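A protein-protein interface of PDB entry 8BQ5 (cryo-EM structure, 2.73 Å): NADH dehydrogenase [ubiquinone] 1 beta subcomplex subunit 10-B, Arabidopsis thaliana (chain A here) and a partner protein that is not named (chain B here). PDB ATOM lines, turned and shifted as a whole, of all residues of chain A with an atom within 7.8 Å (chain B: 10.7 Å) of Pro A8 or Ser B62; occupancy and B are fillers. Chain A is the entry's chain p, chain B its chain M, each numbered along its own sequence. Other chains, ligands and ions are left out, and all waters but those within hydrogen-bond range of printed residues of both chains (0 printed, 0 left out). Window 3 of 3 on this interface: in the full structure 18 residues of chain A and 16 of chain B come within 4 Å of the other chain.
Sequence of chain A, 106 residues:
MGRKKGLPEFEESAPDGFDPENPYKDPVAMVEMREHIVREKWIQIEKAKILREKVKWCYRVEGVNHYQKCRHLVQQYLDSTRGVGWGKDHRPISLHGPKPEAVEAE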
ATOM      1  N   ARG A   3      11.038   3.188  30.985  1.00  0.00           N
ATOM      2  CA  ARG A   3      10.687   2.613  29.694  1.00  0.00           C
ATOM      3  C   ARG A   3      11.375   3.387  28.579  1.00  0.00           C
ATOM      4  O   ARG A   3      11.439   4.619  28.612  1.00  0.00           O
ATOM      5  CB  ARG A   3       9.165   2.615  29.476  1.00  0.00           C
ATOM      6  CG  ARG A   3       8.741   2.814  28.024  1.00  0.00           C
ATOM      7  CD  ARG A   3       7.260   3.126  27.894  1.00  0.00           C
ATOM      8  NE  ARG A   3       6.437   1.928  28.004  1.00  0.00           N
ATOM      9  CZ  ARG A   3       6.153   1.117  26.992  1.00  0.00           C
ATOM     10  NH1 ARG A   3       6.596   1.356  25.769  1.00  0.00           N
ATOM     11  NH2 ARG A   3       5.404   0.041  27.214  1.00  0.00           N
ATOM     12  N   LYS A   4      11.891   2.654  27.596  1.00  0.00           N
ATOM     13  CA  LYS A   4      12.553   3.264  26.453  1.00  0.00           C
ATOM     14  C   LYS A   4      11.545   3.993  25.566  1.00  0.00           C
ATOM     15  O   LYS A   4      10.386   3.591  25.441  1.00  0.00           O
ATOM     16  CB  LYS A   4      13.295   2.199  25.645  1.00  0.00           C
ATOM     17  CG  LYS A   4      14.398   1.494  26.425  1.00  0.00           C
ATOM     18  CD  LYS A   4      15.367   0.763  25.506  1.00  0.00           C
ATOM     19  CE  LYS A   4      16.456   0.063  26.309  1.00  0.00           C
ATOM     20  NZ  LYS A   4      17.379  -0.736  25.454  1.00  0.00           N
ATOM     21  N   LYS A   5      12.005   5.075  24.944  1.00  0.00           N
ATOM     22  CA  LYS A   5      11.146   5.866  24.072  1.00  0.00           C
ATOM     23  C   LYS A   5      10.831   5.107  22.788  1.00  0.00           C
ATOM     24  O   LYS A   5      11.712   4.501  22.174  1.00  0.00           O
ATOM     25  CB  LYS A   5      11.822   7.198  23.750  1.00  0.00           C
ATOM     26  CG  LYS A   5      11.014   8.140  22.877  1.00  0.00           C
ATOM     27  CD  LYS A   5      11.908   9.232  22.312  1.00  0.00           C
ATOM     28  CE  LYS A   5      11.255  10.599  22.413  1.00  0.00           C
ATOM     29  NZ  LYS A   5      10.936  10.959  23.821  1.00  0.00           N
ATOM     30  N   GLY A   6       9.566   5.138  22.387  1.00  0.00           N
ATOM     31  CA  GLY A   6       9.120   4.492  21.169  1.00  0.00           C
ATOM     32  C   GLY A   6       7.788   3.787  21.348  1.00  0.00           C
ATOM     33  O   GLY A   6       7.213   3.735  22.434  1.00  0.00           O
ATOM     34  N   LEU A   7       7.306   3.241  20.235  1.00  0.00           N
ATOM     35  CA  LEU A   7       6.074   2.469  20.244  1.00  0.00           C
ATOM     36  C   LEU A   7       6.299   1.133  20.952  1.00  0.00           C
ATOM     37  O   LEU A   7       7.434   0.657  21.050  1.00  0.00           O
ATOM     38  CB  LEU A   7       5.585   2.226  18.817  1.00  0.00           C
ATOM     39  CG  LEU A   7       5.120   3.443  18.015  1.00  0.00           C
ATOM     40  CD1 LEU A   7       6.276   4.038  17.228  1.00  0.00           C
ATOM     41  CD2 LEU A   7       3.971   3.067  17.086  1.00  0.00           C
ATOM     42  N   PRO A   8       5.239   0.518  21.480  1.00  0.00           N
ATOM     43  CA  PRO A   8       5.396  -0.817  22.067  1.00  0.00           C
ATOM     44  C   PRO A   8       5.724  -1.851  21.001  1.00  0.00           C
ATOM     45  O   PRO A   8       5.283  -1.758  19.855  1.00  0.00           O
ATOM     46  CB  PRO A   8       4.037  -1.096  22.720  1.00  0.00           C
ATOM     47  CG  PRO A   8       3.092  -0.110  22.165  1.00  0.00           C
ATOM     48  CD  PRO A   8       3.843   0.992  21.498  1.00  0.00           C
ATOM     49  N   GLU A   9       6.513  -2.843  21.396  1.00  0.00           N
ATOM     50  CA  GLU A   9       6.910  -3.938  20.522  1.00  0.00           C
ATOM     51  C   GLU A   9       6.334  -5.237  21.064  1.00  0.00           C
ATOM     52  O   GLU A   9       6.390  -5.487  22.272  1.00  0.00           O
ATOM     53  CB  GLU A   9       8.433  -4.041  20.428  1.00  0.00           C
ATOM     54  CG  GLU A   9       9.116  -2.850  19.781  1.00  0.00           C
ATOM     55  CD  GLU A   9       9.641  -3.155  18.391  1.00  0.00           C
ATOM     56  OE1 GLU A   9       9.478  -4.302  17.926  1.00  0.00           O
ATOM     57  OE2 GLU A   9      10.228  -2.246  17.767  1.00  0.00           O
ATOM     58  N   PHE A  10       5.782  -6.057  20.175  1.00  0.00           N
ATOM     59  CA  PHE A  10       5.286  -7.371  20.544  1.00  0.00           C
ATOM     60  C   PHE A  10       5.773  -8.397  19.534  1.00  0.00           C
ATOM     61  O   PHE A  10       6.086  -8.072  18.386  1.00  0.00           O
ATOM     62  CB  PHE A  10       3.755  -7.411  20.632  1.00  0.00           C
ATOM     63  CG  PHE A  10       3.172  -6.377  21.548  1.00  0.00           C
ATOM     64  CD1 PHE A  10       2.911  -6.679  22.874  1.00  0.00           C
ATOM     65  CD2 PHE A  10       2.866  -5.111  21.081  1.00  0.00           C
ATOM     66  CE1 PHE A  10       2.373  -5.733  23.722  1.00  0.00           C
ATOM     67  CE2 PHE A  10       2.324  -4.160  21.925  1.00  0.00           C
ATOM     68  CZ  PHE A  10       2.077  -4.473  23.247  1.00  0.00           C
ATOM     69  N   GLU A  12       5.663 -10.999  16.758  1.00  0.00           N
ATOM     70  CA  GLU A  12       4.747 -10.999  15.624  1.00  0.00           C
ATOM     71  C   GLU A  12       4.022 -12.330  15.474  1.00  0.00           C
ATOM     72  O   GLU A  12       2.903 -12.369  14.950  1.00  0.00           O
ATOM     73  CB  GLU A  12       5.508 -10.667  14.342  1.00  0.00           C
ATOM     74  CG  GLU A  12       6.490  -9.521  14.499  1.00  0.00           C
ATOM     75  CD  GLU A  12       5.825  -8.165  14.379  1.00  0.00           C
ATOM     76  OE1 GLU A  12       6.392  -7.178  14.892  1.00  0.00           O
ATOM     77  OE2 GLU A  12       4.740  -8.085  13.767  1.00  0.00           O
ATOM     78  N   GLU A  35      -3.363 -12.900  24.372  1.00  0.00           N
ATOM     79  CA  GLU A  35      -2.861 -11.545  24.040  1.00  0.00           C
ATOM     80  C   GLU A  35      -2.621 -11.433  22.537  1.00  0.00           C
ATOM     81  O   GLU A  35      -2.977 -10.383  21.970  1.00  0.00           O
ATOM     82  CB  GLU A  35      -1.553 -11.299  24.781  1.00  0.00           C
ATOM     83  CG  GLU A  35      -1.725 -11.213  26.281  1.00  0.00           C
ATOM     84  CD  GLU A  35      -0.410 -11.040  27.018  1.00  0.00           C
ATOM     85  OE1 GLU A  35       0.644 -11.175  26.376  1.00  0.00           O
ATOM     86  OE2 GLU A  35      -0.452 -10.749  28.226  1.00  0.00           O
ATOM     87  N   VAL A  38      -5.911 -11.010  20.616  1.00  0.00           N
ATOM     88  CA  VAL A  38      -6.463  -9.666  20.767  1.00  0.00           C
ATOM     89  C   VAL A  38      -5.752  -8.692  19.836  1.00  0.00           C
ATOM     90  O   VAL A  38      -6.392  -7.888  19.146  1.00  0.00           O
ATOM     91  CB  VAL A  38      -6.368  -9.215  22.237  1.00  0.00           C
ATOM     92  CG1 VAL A  38      -6.342  -7.700  22.333  1.00  0.00           C
ATOM     93  CG2 VAL A  38      -7.519  -9.784  23.041  1.00  0.00           C
ATOM     94  N   ARG A  39      -4.419  -8.760  19.791  1.00  0.00           N
ATOM     95  CA  ARG A  39      -3.657  -7.863  18.929  1.00  0.00           C
ATOM     96  C   ARG A  39      -3.968  -8.116  17.460  1.00  0.00           C
ATOM     97  O   ARG A  39      -4.049  -7.174  16.664  1.00  0.00           O
ATOM     98  CB  ARG A  39      -2.163  -8.027  19.200  1.00  0.00           C
ATOM     99  CG  ARG A  39      -1.526  -6.852  19.926  1.00  0.00           C
ATOM    100  CD  ARG A  39      -0.752  -7.307  21.144  1.00  0.00           C
ATOM    101  NE  ARG A  39       0.077  -8.471  20.865  1.00  0.00           N
ATOM    102  CZ  ARG A  39       0.648  -9.218  21.799  1.00  0.00           C
ATOM    103  NH1 ARG A  39       0.510  -8.943  23.084  1.00  0.00           N
ATOM    104  NH2 ARG A  39       1.377 -10.269  21.433  1.00  0.00           N
ATOM    105  N   TRP B  56      -2.088   7.325  37.587  1.00  0.00           N
ATOM    106  CA  TRP B  56      -2.640   7.392  36.236  1.00  0.00           C
ATOM    107  C   TRP B  56      -1.566   7.760  35.217  1.00  0.00           C
ATOM    108  O   TRP B  56      -1.539   7.212  34.109  1.00  0.00           O
ATOM    109  CB  TRP B  56      -3.788   8.401  36.190  1.00  0.00           C
ATOM    110  CG  TRP B  56      -4.528   8.459  34.881  1.00  0.00           C
ATOM    111  CD1 TRP B  56      -4.361   7.644  33.800  1.00  0.00           C
ATOM    112  CD2 TRP B  56      -5.555   9.389  34.525  1.00  0.00           C
ATOM    113  NE1 TRP B  56      -5.214   8.014  32.790  1.00  0.00           N
ATOM    114  CE2 TRP B  56      -5.961   9.081  33.211  1.00  0.00           C
ATOM    115  CE3 TRP B  56      -6.173  10.453  35.189  1.00  0.00           C
ATOM    116  CZ2 TRP B  56      -6.956   9.796  32.551  1.00  0.00           C
ATOM    117  CZ3 TRP B  56      -7.158  11.161  34.532  1.00  0.00           C
ATOM    118  CH2 TRP B  56      -7.540  10.830  33.226  1.00  0.00           C
ATOM    119  N   ILE B  57      -0.670   8.680  35.577  1.00  0.00           N
ATOM    120  CA  ILE B  57       0.297   9.198  34.610  1.00  0.00           C
ATOM    121  C   ILE B  57       1.211   8.090  34.090  1.00  0.00           C
ATOM    122  O   ILE B  57       1.480   8.004  32.885  1.00  0.00           O
ATOM    123  CB  ILE B  57       1.099  10.354  35.234  1.00  0.00           C
ATOM    124  CG1 ILE B  57       0.277  11.637  35.166  1.00  0.00           C
ATOM    125  CG2 ILE B  57       2.433  10.534  34.529  1.00  0.00           C
ATOM    126  CD1 ILE B  57      -0.264  11.906  33.793  1.00  0.00           C
ATOM    127  N   GLN B  58       1.696   7.226  34.979  1.00  0.00           N
ATOM    128  CA  GLN B  58       2.650   6.183  34.624  1.00  0.00           C
ATOM    129  C   GLN B  58       1.981   4.915  34.101  1.00  0.00           C
ATOM    130  O   GLN B  58       2.606   3.850  34.103  1.00  0.00           O
ATOM    131  CB  GLN B  58       3.523   5.846  35.832  1.00  0.00           C
ATOM    132  CG  GLN B  58       2.744   5.777  37.129  1.00  0.00           C
ATOM    133  CD  GLN B  58       3.603   5.368  38.303  1.00  0.00           C
ATOM    134  OE1 GLN B  58       4.581   6.036  38.631  1.00  0.00           O
ATOM    135  NE2 GLN B  58       3.238   4.269  38.947  1.00  0.00           N
ATOM    136  N   PHE B  59       0.733   5.006  33.650  1.00  0.00           N
ATOM    137  CA  PHE B  59      -0.018   3.831  33.235  1.00  0.00           C
ATOM    138  C   PHE B  59       0.323   3.444  31.800  1.00  0.00           C
ATOM    139  O   PHE B  59       0.476   4.305  30.929  1.00  0.00           O
ATOM    140  CB  PHE B  59      -1.517   4.098  33.366  1.00  0.00           C
ATOM    141  CG  PHE B  59      -2.377   2.906  33.087  1.00  0.00           C
ATOM    142  CD1 PHE B  59      -2.549   1.920  34.042  1.00  0.00           C
ATOM    143  CD2 PHE B  59      -3.025   2.775  31.870  1.00  0.00           C
ATOM    144  CE1 PHE B  59      -3.346   0.826  33.789  1.00  0.00           C
ATOM    145  CE2 PHE B  59      -3.822   1.683  31.610  1.00  0.00           C
ATOM    146  CZ  PHE B  59      -3.982   0.706  32.569  1.00  0.00           C
ATOM    147  N   ASP B  60       0.440   2.139  31.561  1.00  0.00           N
ATOM    148  CA  ASP B  60       0.715   1.590  30.235  1.00  0.00           C
ATOM    149  C   ASP B  60      -0.608   1.088  29.667  1.00  0.00           C
ATOM    150  O   ASP B  60      -1.252   0.213  30.256  1.00  0.00           O
ATOM    151  CB  ASP B  60       1.756   0.472  30.315  1.00  0.00           C
ATOM    152  CG  ASP B  60       2.115  -0.119  28.950  1.00  0.00           C
ATOM    153  OD1 ASP B  60       1.315  -0.033  27.995  1.00  0.00           O
ATOM    154  OD2 ASP B  60       3.223  -0.680  28.835  1.00  0.00           O
ATOM    155  N   SER B  61      -1.001   1.632  28.519  1.00  0.00           N
ATOM    156  CA  SER B  61      -2.255   1.275  27.870  1.00  0.00           C
ATOM    157  C   SER B  61      -2.069   0.258  26.747  1.00  0.00           C
ATOM    158  O   SER B  61      -3.020  -0.012  26.005  1.00  0.00           O
ATOM    159  CB  SER B  61      -2.948   2.535  27.347  1.00  0.00           C
ATOM    160  OG  SER B  61      -2.239   3.096  26.260  1.00  0.00           O
ATOM    161  N   SER B  62      -0.870  -0.311  26.609  1.00  0.00           N
ATOM    162  CA  SER B  62      -0.619  -1.367  25.640  1.00  0.00           C
ATOM    163  C   SER B  62      -0.661  -2.763  26.236  1.00  0.00           C
ATOM    164  O   SER B  62      -0.955  -3.716  25.510  1.00  0.00           O
ATOM    165  CB  SER B  62       0.749  -1.173  24.969  1.00  0.00           C
ATOM    166  OG  SER B  62       1.801  -1.556  25.839  1.00  0.00           O
ATOM    167  N   THR B  63      -0.464  -2.858  27.545  1.00  0.00           N
ATOM    168  CA  THR B  63      -0.326  -4.202  28.148  1.00  0.00           C
ATOM    169  C   THR B  63      -1.636  -4.775  28.682  1.00  0.00           C
ATOM    170  O   THR B  63      -2.546  -3.996  29.026  1.00  0.00           O
ATOM    171  CB  THR B  63       0.759  -4.181  29.232  1.00  0.00           C
ATOM    172  OG1 THR B  63       1.142  -5.533  29.484  1.00  0.00           O
ATOM    173  CG2 THR B  63       0.321  -3.521  30.519  1.00  0.00           C
ATOM    174  N   ALA B  64      -1.708  -6.103  28.746  1.00  0.00           N
ATOM    175  CA  ALA B  64      -2.867  -6.783  29.355  1.00  0.00           C
ATOM    176  C   ALA B  64      -2.413  -7.344  30.702  1.00  0.00           C
ATOM    177  O   ALA B  64      -3.242  -7.931  31.412  1.00  0.00           O
ATOM    178  CB  ALA B  64      -3.313  -7.876  28.432  1.00  0.00           C
ATOM    179  N   LYS B  65      -1.131  -7.168  31.030  1.00  0.00           N
ATOM    180  CA  LYS B  65      -0.570  -7.722  32.283  1.00  0.00           C
ATOM    181  C   LYS B  65      -0.890  -6.747  33.417  1.00  0.00           C
ATOM    182  O   LYS B  65      -0.929  -5.524  33.164  1.00  0.00           O
ATOM    183  CB  LYS B  65       0.933  -7.966  32.109  1.00  0.00           C
ATOM    184  CG  LYS B  65       1.312  -9.345  31.593  1.00  0.00           C
ATOM    185  CD  LYS B  65       1.398  -9.419  30.084  1.00  0.00           C
ATOM    186  CE  LYS B  65       1.976 -10.728  29.592  1.00  0.00           C
ATOM    187  NZ  LYS B  65       3.233 -11.080  30.290  1.00  0.00           N
ATOM    188  N   PHE B  66      -1.131  -7.278  34.610  1.00  0.00           N
ATOM    189  CA  PHE B  66      -1.434  -6.412  35.773  1.00  0.00           C
ATOM    190  C   PHE B  66      -0.251  -5.469  35.971  1.00  0.00           C
ATOM    191  O   PHE B  66       0.912  -5.908  35.880  1.00  0.00           O
ATOM    192  CB  PHE B  66      -1.835  -7.273  36.972  1.00  0.00           C
ATOM    193  CG  PHE B  66      -3.195  -7.899  36.816  1.00  0.00           C
ATOM    194  CD1 PHE B  66      -4.334  -7.111  36.787  1.00  0.00           C
ATOM    195  CD2 PHE B  66      -3.336  -9.267  36.663  1.00  0.00           C
ATOM    196  CE1 PHE B  66      -5.585  -7.684  36.633  1.00  0.00           C
ATOM    197  CE2 PHE B  66      -4.588  -9.838  36.508  1.00  0.00           C
ATOM    198  CZ  PHE B  66      -5.711  -9.046  36.489  1.00  0.00           C
ATOM    199  N   GLN B  67      -0.546  -4.194  36.197  1.00  0.00           N
ATOM    200  CA  GLN B  67       0.539  -3.196  36.281  1.00  0.00           C
ATOM    201  C   GLN B  67       0.843  -2.841  37.730  1.00  0.00           C
ATOM    202  O   GLN B  67      -0.008  -3.115  38.594  1.00  0.00           O
ATOM    203  CB  GLN B  67       0.156  -1.957  35.487  1.00  0.00           C
ATOM    204  CG  GLN B  67       0.296  -2.177  33.996  1.00  0.00           C
ATOM    205  CD  GLN B  67      -0.345  -1.044  33.245  1.00  0.00           C
ATOM    206  OE1 GLN B  67       0.077   0.101  33.353  1.00  0.00           O
ATOM    207  NE2 GLN B  67      -1.383  -1.363  32.493  1.00  0.00           N
ATOM    208  N   ASP B  87      -5.289  -2.566  36.555  1.00  0.00           N
ATOM    209  CA  ASP B  87      -5.289  -2.678  35.102  1.00  0.00           C
ATOM    210  C   ASP B  87      -6.133  -1.535  34.554  1.00  0.00           C
ATOM    211  O   ASP B  87      -6.443  -0.578  35.272  1.00  0.00           O
ATOM    212  CB  ASP B  87      -5.808  -4.056  34.657  1.00  0.00           C
ATOM    213  CG  ASP B  87      -7.007  -4.510  35.461  1.00  0.00           C
ATOM    214  OD1 ASP B  87      -8.079  -4.735  34.858  1.00  0.00           O
ATOM    215  OD2 ASP B  87      -6.882  -4.636  36.695  1.00  0.00           O
ATOM    216  N   GLY B  88      -6.509  -1.630  33.285  1.00  0.00           N
ATOM    217  CA  GLY B  88      -7.395  -0.649  32.703  1.00  0.00           C
ATOM    218  C   GLY B  88      -8.791  -0.633  33.274  1.00  0.00           C
ATOM    219  O   GLY B  88      -9.514   0.348  33.096  1.00  0.00           O
ATOM    220  N   LEU B 478     -11.199   5.875  27.404  1.00  0.00           N
ATOM    221  CA  LEU B 478     -11.301   4.683  26.567  1.00  0.00           C
ATOM    222  C   LEU B 478      -9.936   4.217  26.072  1.00  0.00           C
ATOM    223  O   LEU B 478      -9.746   3.022  25.825  1.00  0.00           O
ATOM    224  CB  LEU B 478     -12.239   4.957  25.392  1.00  0.00           C
ATOM    225  CG  LEU B 478     -13.735   5.038  25.722  1.00  0.00           C
ATOM    226  CD1 LEU B 478     -14.527   5.572  24.540  1.00  0.00           C
ATOM    227  CD2 LEU B 478     -14.272   3.682  26.146  1.00  0.00           C
ATOM    228  N   ASP B 479      -8.981   5.138  25.918  1.00  0.00           N
ATOM    229  CA  ASP B 479      -7.639   4.751  25.496  1.00  0.00           C
ATOM    230  C   ASP B 479      -6.955   3.874  26.537  1.00  0.00           C
ATOM    231  O   ASP B 479      -6.267   2.908  26.188  1.00  0.00           O
ATOM    232  CB  ASP B 479      -6.794   5.992  25.220  1.00  0.00           C
ATOM    233  CG  ASP B 479      -6.972   6.513  23.814  1.00  0.00           C
ATOM    234  OD1 ASP B 479      -7.660   5.840  23.018  1.00  0.00           O
ATOM    235  OD2 ASP B 479      -6.427   7.592  23.506  1.00  0.00           O
ATOM    236  N   CYS B 480      -7.121   4.201  27.817  1.00  0.00           N
ATOM    237  CA  CYS B 480      -6.457   3.467  28.884  1.00  0.00           C
ATOM    238  C   CYS B 480      -7.199   2.205  29.295  1.00  0.00           C
ATOM    239  O   CYS B 480      -6.702   1.466  30.150  1.00  0.00           O
ATOM    240  CB  CYS B 480      -6.276   4.367  30.108  1.00  0.00           C
ATOM    241  SG  CYS B 480      -5.251   5.830  29.825  1.00  0.00           S
ATOM    242  N   MET B 481      -8.369   1.937  28.719  1.00  0.00           N
ATOM    243  CA  MET B 481      -9.169   0.786  29.114  1.00  0.00           C
ATOM    244  C   MET B 481      -9.236  -0.306  28.060  1.00  0.00           C
ATOM    245  O   MET B 481      -9.518  -1.455  28.403  1.00  0.00           O
ATOM    246  CB  MET B 481     -10.601   1.222  29.448  1.00  0.00           C
ATOM    247  CG  MET B 481     -10.746   1.975  30.758  1.00  0.00           C
ATOM    248  SD  MET B 481     -12.294   2.893  30.889  1.00  0.00           S
ATOM    249  CE  MET B 481     -13.078   2.485  29.332  1.00  0.00           C
ATOM    250  N   HIS B 482      -8.962   0.017  26.796  1.00  0.00           N
ATOM    251  CA  HIS B 482      -9.351  -0.867  25.701  1.00  0.00           C
ATOM    252  C   HIS B 482      -8.569  -2.175  25.698  1.00  0.00           C
ATOM    253  O   HIS B 482      -9.119  -3.227  25.357  1.00  0.00           O
ATOM    254  CB  HIS B 482      -9.197  -0.144  24.366  1.00  0.00           C
ATOM    255  CG  HIS B 482     -10.456   0.514  23.900  1.00  0.00           C
ATOM    256  ND1 HIS B 482     -10.463   1.674  23.157  1.00  0.00           N
ATOM    257  CD2 HIS B 482     -11.755   0.181  24.090  1.00  0.00           C
ATOM    258  CE1 HIS B 482     -11.711   2.021  22.900  1.00  0.00           C
ATOM    259  NE2 HIS B 482     -12.515   1.131  23.454  1.00  0.00           N
ATOM    260  N   THR B 483      -7.282  -2.133  26.049  1.00  0.00           N
ATOM    261  CA  THR B 483      -6.488  -3.359  26.053  1.00  0.00           C
ATOM    262  C   THR B 483      -6.960  -4.319  27.139  1.00  0.00           C
ATOM    263  O   THR B 483      -7.094  -5.525  26.905  1.00  0.00           O
ATOM    264  CB  THR B 483      -5.005  -3.033  26.230  1.00  0.00           C
ATOM    265  OG1 THR B 483      -4.551  -2.249  25.121  1.00  0.00           O
ATOM    266  CG2 THR B 483      -4.189  -4.311  26.294  1.00  0.00           C
ATOM    267  N   SER B 484      -7.213  -3.799  28.344  1.00  0.00           N
ATOM    268  CA  SER B 484      -7.748  -4.634  29.414  1.00  0.00           C
ATOM    269  C   SER B 484      -9.160  -5.101  29.087  1.00  0.00           C
ATOM    270  O   SER B 484      -9.545  -6.230  29.407  1.00  0.00           O
ATOM    271  CB  SER B 484      -7.733  -3.871  30.738  1.00  0.00           C
ATOM    272  OG  SER B 484      -6.412  -3.609  31.168  1.00  0.00           O
ATOM    273  N   VAL B 485      -9.955  -4.228  28.465  1.00  0.00           N
ATOM    274  CA  VAL B 485     -11.312  -4.603  28.080  1.00  0.00           C
ATOM    275  C   VAL B 485     -11.281  -5.675  27.000  1.00  0.00           C
ATOM    276  O   VAL B 485     -12.040  -6.650  27.051  1.00  0.00           O
ATOM    277  CB  VAL B 485     -12.098  -3.358  27.626  1.00  0.00           C
ATOM    278  CG1 VAL B 485     -13.319  -3.762  26.820  1.00  0.00           C
ATOM    279  CG2 VAL B 485     -12.504  -2.529  28.828  1.00  0.00           C
ATOM    280  N   SER B 486     -10.400  -5.514  26.009  1.00  0.00           N
ATOM    281  CA  SER B 486     -10.310  -6.485  24.923  1.00  0.00           C
ATOM    282  C   SER B 486      -9.931  -7.862  25.445  1.00  0.00           C
ATOM    283  O   SER B 486     -10.503  -8.874  25.026  1.00  0.00           O
ATOM    284  CB  SER B 486      -9.288  -6.019  23.888  1.00  0.00           C
ATOM    285  OG  SER B 486      -9.806  -4.971  23.096  1.00  0.00           O
ATOM    286  N   ASN B 487      -8.961  -7.919  26.359  1.00  0.00           N
ATOM    287  CA  ASN B 487      -8.525  -9.197  26.902  1.00  0.00           C
ATOM    288  C   ASN B 487      -9.573  -9.801  27.825  1.00  0.00           C
ATOM    289  O   ASN B 487      -9.609 -11.023  28.005  1.00  0.00           O
ATOM    290  CB  ASN B 487      -7.200  -9.023  27.639  1.00  0.00           C
ATOM    291  CG  ASN B 487      -6.009  -9.295  26.752  1.00  0.00           C
ATOM    292  OD1 ASN B 487      -5.539  -8.412  26.040  1.00  0.00           O
ATOM    293  ND2 ASN B 487      -5.513 -10.520  26.786  1.00  0.00           N
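The guanidinium group (NH2) of Arg A3 is in salt-bridge range of the side-chain carboxylate (OD2) of Asp B60.
No residue of chain B comes within 4 Å of Leu A7. Of chain B, only Ser B62 (3.8 Å) comes within 4 Å of Pro A8. No residue of chain B comes within 4 Å of Glu A9. Of the printed residues of chain A, Asp B60 touches Arg A3 (2.8 Å). Ser B61 touches none of the printed residues of chain A. Ser B62 touches two residues of chain A. Printed residues of chain A within 4 Å of Lys B65: Glu A35. Gly B88 touches none of the printed residues of chain A. Of the printed residues of chain A, Ser B486 touches Val A38. The nearest residue of chain B that does not touch Pro A8 is Asp B60 (6.0 Å). The nearest residue of chain A that does not touch Ser B62 is Arg A3 (4.2 Å). The nearest printed residue of chain A that does not touch Ser B486 is Arg A39 (6.9 Å).
The side-chain carboxylate (OD1) of Asp B60 is in hydrogen-bond range of the backbone NH (N) of Thr B63 (3.4 Å). The backbone NH (N) of Asp B60 lies within hydrogen-bond range of the side-chain amide oxygen (OE1) of Gln B67 (2.7 Å). The backbone NH of Lys B65 lies within hydrogen-bond range of the side-chain hydroxyl of Thr B63, 3.2 Å away. O of His B482 lies within hydrogen-bond range of OG of Ser B486 (2.9 Å). The backbone carbonyl oxygen of Thr B483 sits close to the side-chain amide oxygen of Asn B487 (3.4 Å). The guanidinium group of Arg A39 is in salt-bridge range of the side-chain carboxylate of Glu A35 (3.98 Å).
Among the printed residues, merely in contact across the chains: Pro A8 with Ser B62, Phe A10 with Ser B62, Glu A35 with Lys B65, Glu A35 with Asn B487, Val A38 with Ser B486 and Val A38 with Asn B487.
Hydrophobic or aromatic side chains of chain A that line the printed part of chain B: Pro A8, Phe A10 and Val A38. Of the 24 printed residues of chain B, 5 touch a printed residue of chain A. Among the printed residues, 7 pairs touch across the chains. Among the printed residues, Asp or Glu carboxylates within 4 Å of a Lys or Arg side-chain nitrogen of the other chain: Arg A3 with Asp B60.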
